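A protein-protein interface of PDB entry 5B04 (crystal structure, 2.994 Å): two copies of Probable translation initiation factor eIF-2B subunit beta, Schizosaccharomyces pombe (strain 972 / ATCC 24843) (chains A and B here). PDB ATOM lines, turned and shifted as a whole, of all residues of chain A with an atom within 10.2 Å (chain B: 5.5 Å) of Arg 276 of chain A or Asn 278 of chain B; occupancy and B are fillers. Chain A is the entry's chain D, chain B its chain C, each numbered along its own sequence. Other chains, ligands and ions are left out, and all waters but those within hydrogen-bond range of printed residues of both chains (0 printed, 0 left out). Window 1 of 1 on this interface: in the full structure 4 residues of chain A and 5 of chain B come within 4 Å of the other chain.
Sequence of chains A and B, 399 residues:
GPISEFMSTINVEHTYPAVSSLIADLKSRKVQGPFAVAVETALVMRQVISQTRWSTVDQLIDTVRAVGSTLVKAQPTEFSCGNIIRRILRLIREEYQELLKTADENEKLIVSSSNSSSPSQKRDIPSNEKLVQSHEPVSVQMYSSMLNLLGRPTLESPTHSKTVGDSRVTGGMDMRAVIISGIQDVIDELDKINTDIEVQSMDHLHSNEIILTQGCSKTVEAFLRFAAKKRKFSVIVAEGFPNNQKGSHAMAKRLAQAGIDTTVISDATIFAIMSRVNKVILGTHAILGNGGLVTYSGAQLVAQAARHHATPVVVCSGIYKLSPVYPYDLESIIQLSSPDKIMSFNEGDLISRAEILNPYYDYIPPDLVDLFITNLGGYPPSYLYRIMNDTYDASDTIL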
ATOM      1  N   ASN A 208      24.838  -9.402  -1.702  1.00  0.00           N
ATOM      2  CA  ASN A 208      25.930  -8.651  -2.323  1.00  0.00           C
ATOM      3  C   ASN A 208      25.522  -7.869  -3.571  1.00  0.00           C
ATOM      4  O   ASN A 208      26.373  -7.317  -4.266  1.00  0.00           O
ATOM      5  CB  ASN A 208      27.090  -9.591  -2.659  1.00  0.00           C
ATOM      6  CG  ASN A 208      27.537 -10.409  -1.466  1.00  0.00           C
ATOM      7  OD1 ASN A 208      27.379 -11.629  -1.442  1.00  0.00           O
ATOM      8  ND2 ASN A 208      28.095  -9.739  -0.465  1.00  0.00           N
ATOM      9  N   GLU A 209      24.224  -7.818  -3.850  1.00  0.00           N
ATOM     10  CA  GLU A 209      23.718  -6.992  -4.938  1.00  0.00           C
ATOM     11  C   GLU A 209      23.619  -5.540  -4.490  1.00  0.00           C
ATOM     12  O   GLU A 209      23.472  -5.259  -3.301  1.00  0.00           O
ATOM     13  CB  GLU A 209      22.350  -7.485  -5.418  1.00  0.00           C
ATOM     14  CG  GLU A 209      22.384  -8.764  -6.237  1.00  0.00           C
ATOM     15  CD  GLU A 209      21.026  -9.115  -6.817  1.00  0.00           C
ATOM     16  OE1 GLU A 209      20.074  -8.328  -6.624  1.00  0.00           O
ATOM     17  OE2 GLU A 209      20.908 -10.176  -7.467  1.00  0.00           O
ATOM     18  N   ILE A 210      23.704  -4.620  -5.444  1.00  0.00           N
ATOM     19  CA  ILE A 210      23.528  -3.204  -5.150  1.00  0.00           C
ATOM     20  C   ILE A 210      22.235  -2.701  -5.780  1.00  0.00           C
ATOM     21  O   ILE A 210      22.017  -2.857  -6.982  1.00  0.00           O
ATOM     22  CB  ILE A 210      24.714  -2.363  -5.651  1.00  0.00           C
ATOM     23  CG1 ILE A 210      25.993  -2.764  -4.916  1.00  0.00           C
ATOM     24  CG2 ILE A 210      24.438  -0.881  -5.454  1.00  0.00           C
ATOM     25  CD1 ILE A 210      27.198  -1.924  -5.280  1.00  0.00           C
ATOM     26  N   ILE A 211      21.378  -2.103  -4.959  1.00  0.00           N
ATOM     27  CA  ILE A 211      20.065  -1.657  -5.407  1.00  0.00           C
ATOM     28  C   ILE A 211      19.918  -0.142  -5.302  1.00  0.00           C
ATOM     29  O   ILE A 211      20.312   0.459  -4.302  1.00  0.00           O
ATOM     30  CB  ILE A 211      18.942  -2.331  -4.592  1.00  0.00           C
ATOM     31  CG1 ILE A 211      19.171  -3.840  -4.513  1.00  0.00           C
ATOM     32  CG2 ILE A 211      17.578  -2.020  -5.189  1.00  0.00           C
ATOM     33  CD1 ILE A 211      19.177  -4.528  -5.860  1.00  0.00           C
ATOM     34  N   LEU A 212      19.356   0.471  -6.337  1.00  0.00           N
ATOM     35  CA  LEU A 212      19.094   1.905  -6.319  1.00  0.00           C
ATOM     36  C   LEU A 212      17.602   2.183  -6.170  1.00  0.00           C
ATOM     37  O   LEU A 212      16.777   1.596  -6.868  1.00  0.00           O
ATOM     38  CB  LEU A 212      19.625   2.574  -7.587  1.00  0.00           C
ATOM     39  CG  LEU A 212      19.432   4.092  -7.641  1.00  0.00           C
ATOM     40  CD1 LEU A 212      20.271   4.777  -6.575  1.00  0.00           C
ATOM     41  CD2 LEU A 212      19.763   4.638  -9.020  1.00  0.00           C
ATOM     42  N   SER A 234      23.008  -4.450  -0.404  1.00  0.00           N
ATOM     43  CA  SER A 234      23.209  -3.013  -0.244  1.00  0.00           C
ATOM     44  C   SER A 234      22.154  -2.205  -0.991  1.00  0.00           C
ATOM     45  O   SER A 234      21.680  -2.613  -2.052  1.00  0.00           O
ATOM     46  CB  SER A 234      24.605  -2.615  -0.726  1.00  0.00           C
ATOM     47  OG  SER A 234      25.607  -3.388  -0.088  1.00  0.00           O
ATOM     48  N   VAL A 235      21.790  -1.055  -0.430  1.00  0.00           N
ATOM     49  CA  VAL A 235      20.802  -0.180  -1.051  1.00  0.00           C
ATOM     50  C   VAL A 235      21.279   1.267  -1.095  1.00  0.00           C
ATOM     51  O   VAL A 235      21.642   1.845  -0.071  1.00  0.00           O
ATOM     52  CB  VAL A 235      19.450  -0.232  -0.308  1.00  0.00           C
ATOM     53  CG1 VAL A 235      18.518   0.856  -0.824  1.00  0.00           C
ATOM     54  CG2 VAL A 235      18.810  -1.603  -0.455  1.00  0.00           C
ATOM     55  N   ILE A 236      21.281   1.846  -2.291  1.00  0.00           N
ATOM     56  CA  ILE A 236      21.572   3.263  -2.449  1.00  0.00           C
ATOM     57  C   ILE A 236      20.266   4.036  -2.569  1.00  0.00           C
ATOM     58  O   ILE A 236      19.473   3.794  -3.479  1.00  0.00           O
ATOM     59  CB  ILE A 236      22.450   3.539  -3.682  1.00  0.00           C
ATOM     60  CG1 ILE A 236      23.759   2.751  -3.593  1.00  0.00           C
ATOM     61  CG2 ILE A 236      22.731   5.027  -3.810  1.00  0.00           C
ATOM     62  CD1 ILE A 236      24.703   3.005  -4.748  1.00  0.00           C
ATOM     63  N   THR A 269      23.918  12.564  -7.917  1.00  0.00           N
ATOM     64  CA  THR A 269      24.880  11.471  -7.821  1.00  0.00           C
ATOM     65  C   THR A 269      24.350  10.209  -8.507  1.00  0.00           C
ATOM     66  O   THR A 269      25.091   9.248  -8.723  1.00  0.00           O
ATOM     67  CB  THR A 269      25.217  11.160  -6.343  1.00  0.00           C
ATOM     68  OG1 THR A 269      25.438  12.385  -5.634  1.00  0.00           O
ATOM     69  CG2 THR A 269      26.464  10.292  -6.230  1.00  0.00           C
ATOM     70  N   ILE A 270      23.067  10.232  -8.862  1.00  0.00           N
ATOM     71  CA  ILE A 270      22.379   9.076  -9.441  1.00  0.00           C
ATOM     72  C   ILE A 270      23.124   8.447 -10.623  1.00  0.00           C
ATOM     73  O   ILE A 270      23.271   7.227 -10.692  1.00  0.00           O
ATOM     74  CB  ILE A 270      20.953   9.462  -9.892  1.00  0.00           C
ATOM     75  CG1 ILE A 270      20.055   9.672  -8.671  1.00  0.00           C
ATOM     76  CG2 ILE A 270      20.358   8.391 -10.793  1.00  0.00           C
ATOM     77  CD1 ILE A 270      18.662  10.140  -9.011  1.00  0.00           C
ATOM     78  N   PHE A 271      23.604   9.280 -11.540  1.00  0.00           N
ATOM     79  CA  PHE A 271      24.319   8.779 -12.710  1.00  0.00           C
ATOM     80  C   PHE A 271      25.681   8.203 -12.333  1.00  0.00           C
ATOM     81  O   PHE A 271      26.078   7.153 -12.838  1.00  0.00           O
ATOM     82  CB  PHE A 271      24.496   9.891 -13.748  1.00  0.00           C
ATOM     83  CG  PHE A 271      25.010   9.406 -15.079  1.00  0.00           C
ATOM     84  CD1 PHE A 271      26.369   9.236 -15.297  1.00  0.00           C
ATOM     85  CD2 PHE A 271      24.132   9.130 -16.115  1.00  0.00           C
ATOM     86  CE1 PHE A 271      26.840   8.793 -16.520  1.00  0.00           C
ATOM     87  CE2 PHE A 271      24.598   8.687 -17.340  1.00  0.00           C
ATOM     88  CZ  PHE A 271      25.953   8.520 -17.542  1.00  0.00           C
ATOM     89  N   ALA A 272      26.391   8.897 -11.450  1.00  0.00           N
ATOM     90  CA  ALA A 272      27.769   8.550 -11.111  1.00  0.00           C
ATOM     91  C   ALA A 272      27.904   7.157 -10.501  1.00  0.00           C
ATOM     92  O   ALA A 272      28.864   6.440 -10.783  1.00  0.00           O
ATOM     93  CB  ALA A 272      28.349   9.590 -10.164  1.00  0.00           C
ATOM     94  N   ILE A 273      26.942   6.773  -9.670  1.00  0.00           N
ATOM     95  CA  ILE A 273      26.996   5.486  -8.984  1.00  0.00           C
ATOM     96  C   ILE A 273      26.298   4.385  -9.777  1.00  0.00           C
ATOM     97  O   ILE A 273      26.417   3.204  -9.450  1.00  0.00           O
ATOM     98  CB  ILE A 273      26.365   5.575  -7.577  1.00  0.00           C
ATOM     99  CG1 ILE A 273      24.949   6.153  -7.651  1.00  0.00           C
ATOM    100  CG2 ILE A 273      27.227   6.428  -6.662  1.00  0.00           C
ATOM    101  CD1 ILE A 273      23.845   5.112  -7.653  1.00  0.00           C
ATOM    102  N   MET A 274      25.578   4.785 -10.821  1.00  0.00           N
ATOM    103  CA  MET A 274      24.734   3.874 -11.593  1.00  0.00           C
ATOM    104  C   MET A 274      25.496   2.682 -12.170  1.00  0.00           C
ATOM    105  O   MET A 274      24.941   1.593 -12.310  1.00  0.00           O
ATOM    106  CB  MET A 274      24.051   4.638 -12.729  1.00  0.00           C
ATOM    107  CG  MET A 274      22.833   3.941 -13.306  1.00  0.00           C
ATOM    108  SD  MET A 274      21.470   3.871 -12.131  1.00  0.00           S
ATOM    109  CE  MET A 274      21.242   2.105 -12.006  1.00  0.00           C
ATOM    110  N   SER A 275      26.767   2.896 -12.496  1.00  0.00           N
ATOM    111  CA  SER A 275      27.586   1.872 -13.140  1.00  0.00           C
ATOM    112  C   SER A 275      27.826   0.651 -12.251  1.00  0.00           C
ATOM    113  O   SER A 275      28.157  -0.425 -12.747  1.00  0.00           O
ATOM    114  CB  SER A 275      28.930   2.467 -13.566  1.00  0.00           C
ATOM    115  OG  SER A 275      29.648   2.962 -12.449  1.00  0.00           O
ATOM    116  N   ARG A 276      27.657   0.821 -10.944  1.00  0.00           N
ATOM    117  CA  ARG A 276      27.908  -0.259  -9.994  1.00  0.00           C
ATOM    118  C   ARG A 276      26.615  -0.849  -9.437  1.00  0.00           C
ATOM    119  O   ARG A 276      26.646  -1.716  -8.563  1.00  0.00           O
ATOM    120  CB  ARG A 276      28.788   0.240  -8.848  1.00  0.00           C
ATOM    121  CG  ARG A 276      30.225   0.534  -9.249  1.00  0.00           C
ATOM    122  CD  ARG A 276      31.110  -0.694  -9.096  1.00  0.00           C
ATOM    123  NE  ARG A 276      32.459  -0.462  -9.603  1.00  0.00           N
ATOM    124  CZ  ARG A 276      33.433   0.117  -8.908  1.00  0.00           C
ATOM    125  NH1 ARG A 276      33.211   0.531  -7.669  1.00  0.00           N
ATOM    126  NH2 ARG A 276      34.630   0.286  -9.454  1.00  0.00           N
ATOM    127  N   VAL A 277      25.480  -0.378  -9.947  1.00  0.00           N
ATOM    128  CA  VAL A 277      24.178  -0.832  -9.468  1.00  0.00           C
ATOM    129  C   VAL A 277      23.686  -2.047 -10.248  1.00  0.00           C
ATOM    130  O   VAL A 277      23.713  -2.058 -11.480  1.00  0.00           O
ATOM    131  CB  VAL A 277      23.125   0.290  -9.564  1.00  0.00           C
ATOM    132  CG1 VAL A 277      21.780  -0.192  -9.043  1.00  0.00           C
ATOM    133  CG2 VAL A 277      23.586   1.520  -8.802  1.00  0.00           C
ATOM    134  N   ASN A 278      23.236  -3.067  -9.525  1.00  0.00           N
ATOM    135  CA  ASN A 278      22.717  -4.280 -10.147  1.00  0.00           C
ATOM    136  C   ASN A 278      21.273  -4.137 -10.613  1.00  0.00           C
ATOM    137  O   ASN A 278      20.886  -4.692 -11.641  1.00  0.00           O
ATOM    138  CB  ASN A 278      22.818  -5.459  -9.177  1.00  0.00           C
ATOM    139  CG  ASN A 278      24.248  -5.896  -8.936  1.00  0.00           C
ATOM    140  OD1 ASN A 278      24.861  -5.530  -7.934  1.00  0.00           O
ATOM    141  ND2 ASN A 278      24.786  -6.687  -9.857  1.00  0.00           N
ATOM    142  N   LYS A 279      20.478  -3.391  -9.853  1.00  0.00           N
ATOM    143  CA  LYS A 279      19.041  -3.339 -10.089  1.00  0.00           C
ATOM    144  C   LYS A 279      18.412  -2.059  -9.550  1.00  0.00           C
ATOM    145  O   LYS A 279      18.788  -1.573  -8.483  1.00  0.00           O
ATOM    146  CB  LYS A 279      18.370  -4.553  -9.447  1.00  0.00           C
ATOM    147  CG  LYS A 279      17.323  -5.235 -10.306  1.00  0.00           C
ATOM    148  CD  LYS A 279      16.938  -6.576  -9.702  1.00  0.00           C
ATOM    149  CE  LYS A 279      18.165  -7.456  -9.509  1.00  0.00           C
ATOM    150  NZ  LYS A 279      17.827  -8.781  -8.924  1.00  0.00           N
ATOM    151  N   VAL A 280      17.453  -1.518 -10.294  1.00  0.00           N
ATOM    152  CA  VAL A 280      16.677  -0.375  -9.828  1.00  0.00           C
ATOM    153  C   VAL A 280      15.279  -0.823  -9.419  1.00  0.00           C
ATOM    154  O   VAL A 280      14.558  -1.441 -10.204  1.00  0.00           O
ATOM    155  CB  VAL A 280      16.568   0.725 -10.903  1.00  0.00           C
ATOM    156  CG1 VAL A 280      15.391   1.645 -10.612  1.00  0.00           C
ATOM    157  CG2 VAL A 280      17.857   1.520 -10.976  1.00  0.00           C
ATOM    158  N   ALA A 305      19.080   7.160 -16.517  1.00  0.00           N
ATOM    159  CA  ALA A 305      20.433   6.727 -16.180  1.00  0.00           C
ATOM    160  C   ALA A 305      20.543   5.206 -16.159  1.00  0.00           C
ATOM    161  O   ALA A 305      21.595   4.649 -16.468  1.00  0.00           O
ATOM    162  CB  ALA A 305      20.855   7.303 -14.837  1.00  0.00           C
ATOM    163  N   ALA A 306      19.454   4.538 -15.795  1.00  0.00           N
ATOM    164  CA  ALA A 306      19.435   3.081 -15.753  1.00  0.00           C
ATOM    165  C   ALA A 306      19.478   2.495 -17.160  1.00  0.00           C
ATOM    166  O   ALA A 306      20.220   1.548 -17.424  1.00  0.00           O
ATOM    167  CB  ALA A 306      18.205   2.586 -15.011  1.00  0.00           C
ATOM    168  N   HIS A 309      22.838   2.672 -18.629  1.00  0.00           N
ATOM    169  CA  HIS A 309      23.820   1.770 -18.035  1.00  0.00           C
ATOM    170  C   HIS A 309      23.365   0.315 -18.106  1.00  0.00           C
ATOM    171  O   HIS A 309      23.953  -0.558 -17.467  1.00  0.00           O
ATOM    172  CB  HIS A 309      24.093   2.162 -16.580  1.00  0.00           C
ATOM    173  CG  HIS A 309      24.873   3.431 -16.432  1.00  0.00           C
ATOM    174  ND1 HIS A 309      26.111   3.476 -15.829  1.00  0.00           N
ATOM    175  CD2 HIS A 309      24.593   4.700 -16.810  1.00  0.00           C
ATOM    176  CE1 HIS A 309      26.560   4.719 -15.840  1.00  0.00           C
ATOM    177  NE2 HIS A 309      25.657   5.481 -16.431  1.00  0.00           N
ATOM    178  N   ALA A 310      22.312   0.073 -18.887  1.00  0.00           N
ATOM    179  CA  ALA A 310      21.752  -1.265 -19.087  1.00  0.00           C
ATOM    180  C   ALA A 310      21.304  -1.919 -17.780  1.00  0.00           C
ATOM    181  O   ALA A 310      21.314  -3.143 -17.658  1.00  0.00           O
ATOM    182  CB  ALA A 310      22.755  -2.159 -19.806  1.00  0.00           C
ATOM    183  N   THR A 311      20.908  -1.100 -16.812  1.00  0.00           N
ATOM    184  CA  THR A 311      20.418  -1.604 -15.534  1.00  0.00           C
ATOM    185  C   THR A 311      18.903  -1.781 -15.575  1.00  0.00           C
ATOM    186  O   THR A 311      18.179  -0.861 -15.957  1.00  0.00           O
ATOM    187  CB  THR A 311      20.791  -0.660 -14.374  1.00  0.00           C
ATOM    188  OG1 THR A 311      22.207  -0.445 -14.365  1.00  0.00           O
ATOM    189  CG2 THR A 311      20.363  -1.251 -13.037  1.00  0.00           C
ATOM    190  N   PRO A 312      18.419  -2.971 -15.188  1.00  0.00           N
ATOM    191  CA  PRO A 312      16.982  -3.271 -15.189  1.00  0.00           C
ATOM    192  C   PRO A 312      16.181  -2.408 -14.214  1.00  0.00           C
ATOM    193  O   PRO A 312      16.618  -2.174 -13.086  1.00  0.00           O
ATOM    194  CB  PRO A 312      16.930  -4.746 -14.771  1.00  0.00           C
ATOM    195  CG  PRO A 312      18.225  -4.995 -14.073  1.00  0.00           C
ATOM    196  CD  PRO A 312      19.223  -4.134 -14.779  1.00  0.00           C
ATOM    197  N   HIS B 206      40.847  -2.076 -10.189  1.00  0.00           N
ATOM    198  CA  HIS B 206      40.683  -1.796  -8.769  1.00  0.00           C
ATOM    199  C   HIS B 206      40.167  -3.023  -8.028  1.00  0.00           C
ATOM    200  O   HIS B 206      39.795  -4.021  -8.645  1.00  0.00           O
ATOM    201  CB  HIS B 206      39.744  -0.608  -8.564  1.00  0.00           C
ATOM    202  CG  HIS B 206      40.302   0.690  -9.060  1.00  0.00           C
ATOM    203  ND1 HIS B 206      40.890   1.616  -8.225  1.00  0.00           N
ATOM    204  CD2 HIS B 206      40.370   1.212 -10.307  1.00  0.00           C
ATOM    205  CE1 HIS B 206      41.292   2.655  -8.935  1.00  0.00           C
ATOM    206  NE2 HIS B 206      40.988   2.436 -10.201  1.00  0.00           N
ATOM    207  N   ASN B 208      38.062  -5.774  -5.958  1.00  0.00           N
ATOM    208  CA  ASN B 208      36.714  -6.344  -5.989  1.00  0.00           C
ATOM    209  C   ASN B 208      35.948  -6.105  -7.290  1.00  0.00           C
ATOM    210  O   ASN B 208      34.752  -6.385  -7.368  1.00  0.00           O
ATOM    211  CB  ASN B 208      35.894  -5.816  -4.809  1.00  0.00           C
ATOM    212  CG  ASN B 208      36.458  -6.248  -3.470  1.00  0.00           C
ATOM    213  OD1 ASN B 208      37.343  -5.596  -2.915  1.00  0.00           O
ATOM    214  ND2 ASN B 208      35.951  -7.358  -2.945  1.00  0.00           N
ATOM    215  N   GLU B 209      36.633  -5.599  -8.310  1.00  0.00           N
ATOM    216  CA  GLU B 209      36.036  -5.497  -9.637  1.00  0.00           C
ATOM    217  C   GLU B 209      36.080  -6.856 -10.325  1.00  0.00           C
ATOM    218  O   GLU B 209      36.872  -7.722  -9.952  1.00  0.00           O
ATOM    219  CB  GLU B 209      36.755  -4.448 -10.490  1.00  0.00           C
ATOM    220  CG  GLU B 209      36.340  -3.011 -10.211  1.00  0.00           C
ATOM    221  CD  GLU B 209      36.824  -2.049 -11.282  1.00  0.00           C
ATOM    222  OE1 GLU B 209      37.795  -2.386 -11.993  1.00  0.00           O
ATOM    223  OE2 GLU B 209      36.232  -0.957 -11.417  1.00  0.00           O
ATOM    224  N   ILE B 210      35.224  -7.044 -11.324  1.00  0.00           N
ATOM    225  CA  ILE B 210      35.222  -8.276 -12.101  1.00  0.00           C
ATOM    226  C   ILE B 210      35.606  -7.993 -13.549  1.00  0.00           C
ATOM    227  O   ILE B 210      34.955  -7.202 -14.231  1.00  0.00           O
ATOM    228  CB  ILE B 210      33.853  -8.976 -12.057  1.00  0.00           C
ATOM    229  CG1 ILE B 210      33.573  -9.497 -10.648  1.00  0.00           C
ATOM    230  CG2 ILE B 210      33.807 -10.120 -13.059  1.00  0.00           C
ATOM    231  CD1 ILE B 210      32.310 -10.324 -10.542  1.00  0.00           C
ATOM    232  N   ILE B 211      36.668  -8.646 -14.008  1.00  0.00           N
ATOM    233  CA  ILE B 211      37.197  -8.404 -15.345  1.00  0.00           C
ATOM    234  C   ILE B 211      37.004  -9.604 -16.265  1.00  0.00           C
ATOM    235  O   ILE B 211      37.392 -10.722 -15.930  1.00  0.00           O
ATOM    236  CB  ILE B 211      38.694  -8.054 -15.296  1.00  0.00           C
ATOM    237  CG1 ILE B 211      38.940  -6.916 -14.306  1.00  0.00           C
ATOM    238  CG2 ILE B 211      39.204  -7.692 -16.682  1.00  0.00           C
ATOM    239  CD1 ILE B 211      38.152  -5.661 -14.613  1.00  0.00           C
ATOM    240  N   ARG B 276      27.470  -9.112 -14.533  1.00  0.00           N
ATOM    241  CA  ARG B 276      28.239  -8.857 -13.321  1.00  0.00           C
ATOM    242  C   ARG B 276      29.689  -8.507 -13.647  1.00  0.00           C
ATOM    243  O   ARG B 276      30.563  -8.586 -12.784  1.00  0.00           O
ATOM    244  CB  ARG B 276      28.189 -10.069 -12.387  1.00  0.00           C
ATOM    245  CG  ARG B 276      26.787 -10.603 -12.139  1.00  0.00           C
ATOM    246  CD  ARG B 276      25.946  -9.651 -11.302  1.00  0.00           C
ATOM    247  NE  ARG B 276      25.908 -10.043  -9.895  1.00  0.00           N
ATOM    248  CZ  ARG B 276      26.599  -9.444  -8.930  1.00  0.00           C
ATOM    249  NH1 ARG B 276      27.383  -8.414  -9.214  1.00  0.00           N
ATOM    250  NH2 ARG B 276      26.499  -9.871  -7.679  1.00  0.00           N
ATOM    251  N   VAL B 277      29.938  -8.124 -14.894  1.00  0.00           N
ATOM    252  CA  VAL B 277      31.281  -7.750 -15.325  1.00  0.00           C
ATOM    253  C   VAL B 277      31.424  -6.236 -15.430  1.00  0.00           C
ATOM    254  O   VAL B 277      30.600  -5.568 -16.056  1.00  0.00           O
ATOM    255  CB  VAL B 277      31.642  -8.382 -16.685  1.00  0.00           C
ATOM    256  CG1 VAL B 277      33.008  -7.899 -17.148  1.00  0.00           C
ATOM    257  CG2 VAL B 277      31.616  -9.897 -16.595  1.00  0.00           C
ATOM    258  N   ASN B 278      32.476  -5.703 -14.815  1.00  0.00           N
ATOM    259  CA  ASN B 278      32.747  -4.272 -14.854  1.00  0.00           C
ATOM    260  C   ASN B 278      33.441  -3.844 -16.141  1.00  0.00           C
ATOM    261  O   ASN B 278      33.050  -2.861 -16.771  1.00  0.00           O
ATOM    262  CB  ASN B 278      33.600  -3.858 -13.653  1.00  0.00           C
ATOM    263  CG  ASN B 278      32.873  -4.027 -12.336  1.00  0.00           C
ATOM    264  OD1 ASN B 278      33.239  -4.867 -11.515  1.00  0.00           O
ATOM    265  ND2 ASN B 278      31.839  -3.221 -12.123  1.00  0.00           N
ATOM    266  N   LYS B 279      34.476  -4.585 -16.524  1.00  0.00           N
ATOM    267  CA  LYS B 279      35.299  -4.213 -17.669  1.00  0.00           C
ATOM    268  C   LYS B 279      35.706  -5.415 -18.512  1.00  0.00           C
ATOM    269  O   LYS B 279      35.953  -6.502 -17.989  1.00  0.00           O
ATOM    270  CB  LYS B 279      36.557  -3.475 -17.201  1.00  0.00           C
ATOM    271  CG  LYS B 279      36.301  -2.096 -16.618  1.00  0.00           C
ATOM    272  CD  LYS B 279      37.510  -1.590 -15.848  1.00  0.00           C
ATOM    273  CE  LYS B 279      37.299  -0.162 -15.373  1.00  0.00           C
ATOM    274  NZ  LYS B 279      35.989   0.008 -14.685  1.00  0.00           N
ATOM    275  N   VAL B 280      35.775  -5.207 -19.822  1.00  0.00           N
ATOM    276  CA  VAL B 280      36.337  -6.196 -20.731  1.00  0.00           C
ATOM    277  C   VAL B 280      37.747  -5.776 -21.127  1.00  0.00           C
ATOM    278  O   VAL B 280      37.960  -4.664 -21.611  1.00  0.00           O
ATOM    279  CB  VAL B 280      35.475  -6.374 -21.998  1.00  0.00           C
ATOM    280  CG1 VAL B 280      36.313  -6.905 -23.153  1.00  0.00           C
ATOM    281  CG2 VAL B 280      34.307  -7.298 -21.717  1.00  0.00           C
ATOM    282  N   THR B 311      28.920  -2.613 -21.081  1.00  0.00           N
ATOM    283  CA  THR B 311      30.195  -2.828 -20.408  1.00  0.00           C
ATOM    284  C   THR B 311      31.354  -2.343 -21.277  1.00  0.00           C
ATOM    285  O   THR B 311      31.447  -2.706 -22.450  1.00  0.00           O
ATOM    286  CB  THR B 311      30.402  -4.314 -20.059  1.00  0.00           C
ATOM    287  OG1 THR B 311      29.327  -4.766 -19.226  1.00  0.00           O
ATOM    288  CG2 THR B 311      31.723  -4.517 -19.328  1.00  0.00           C
ATOM    289  N   PRO B 312      32.238  -1.512 -20.700  1.00  0.00           N
ATOM    290  CA  PRO B 312      33.402  -0.959 -21.403  1.00  0.00           C
ATOM    291  C   PRO B 312      34.344  -2.029 -21.952  1.00  0.00           C
ATOM    292  O   PRO B 312      34.615  -3.023 -21.278  1.00  0.00           O
ATOM    293  CB  PRO B 312      34.106  -0.134 -20.321  1.00  0.00           C
ATOM    294  CG  PRO B 312      33.032   0.212 -19.355  1.00  0.00           C
ATOM    295  CD  PRO B 312      32.115  -0.971 -19.335  1.00  0.00           C
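Of the printed residues of chain B, Arg 276 of chain A touches Glu 209 (2.8 Å) and Asn 278 (3.8 Å). Of the printed residues of chain A, Asn 278 of chain B touches Arg 276. No residue of chain A comes within 4 Å of Ile 210 of chain B. No residue of chain A comes within 4 Å of Lys 279 of chain B. No residue of chain A comes within 4 Å of Thr 311 of chain B. No residue of chain A comes within 4 Å of Pro 312 of chain B. Of the printed residues of chain B, Asn 278 of chain A touches Arg 276. Printed residues of chain A within 4 Å of Arg 276 of chain B: Asn 278. The nearest residue of chain A that does not touch Asn 278 of chain B is Ser 275 of chain A (4.7 Å). The nearest printed residue of chain B that does not touch Asn 278 of chain A is Val 277 of chain B (7.3 Å).
Among the printed residues, pairs that only touch across the chains: Arg 276 of chain A with Asn 278 of chain B (3.8 Å).
Arg 276 of chain A touches Glu 209 of chain B, but with the chains exchanged Glu 209 of chain A does not touch Arg 276 of chain B (4.5 Å). Arg 276 of chain A touches Asn 278 of chain B, and with the chains exchanged Asn 278 of chain A touches Arg 276 of chain B. 11 positions are printed for both chains.
Printed residues of chain B that touch a printed residue of chain A: Glu 209, Arg 276 and Asn 278. Among the printed residues, Asp or Glu carboxylates within 4 Å of a Lys or Arg side-chain nitrogen of the other chain: Arg 276 of chain A with Glu 209 of chain B (2.8 Å).
The side-chain carboxylate (OE2) of Glu 209 of chain B is in salt-bridge range of the side-chain amino group (NZ) of Lys 279 of chain B, at 3.4 Å. N of Ile 210 of chain B is in hydrogen-bond range of OD1 of Asn 278 of chain B (3.0 Å). O of Ile 210 of chain A lies within hydrogen-bond range of N of Asn 278 of chain A, 2.8 Å away.
NH2 of Arg 276 of chain A is in salt-bridge range of OE2 of Glu 209 of chain B, 2.8 Å away. NH1 of Arg 276 of chain B sits close to ND2 of Asn 278 of chain A, 3.2 Å away.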
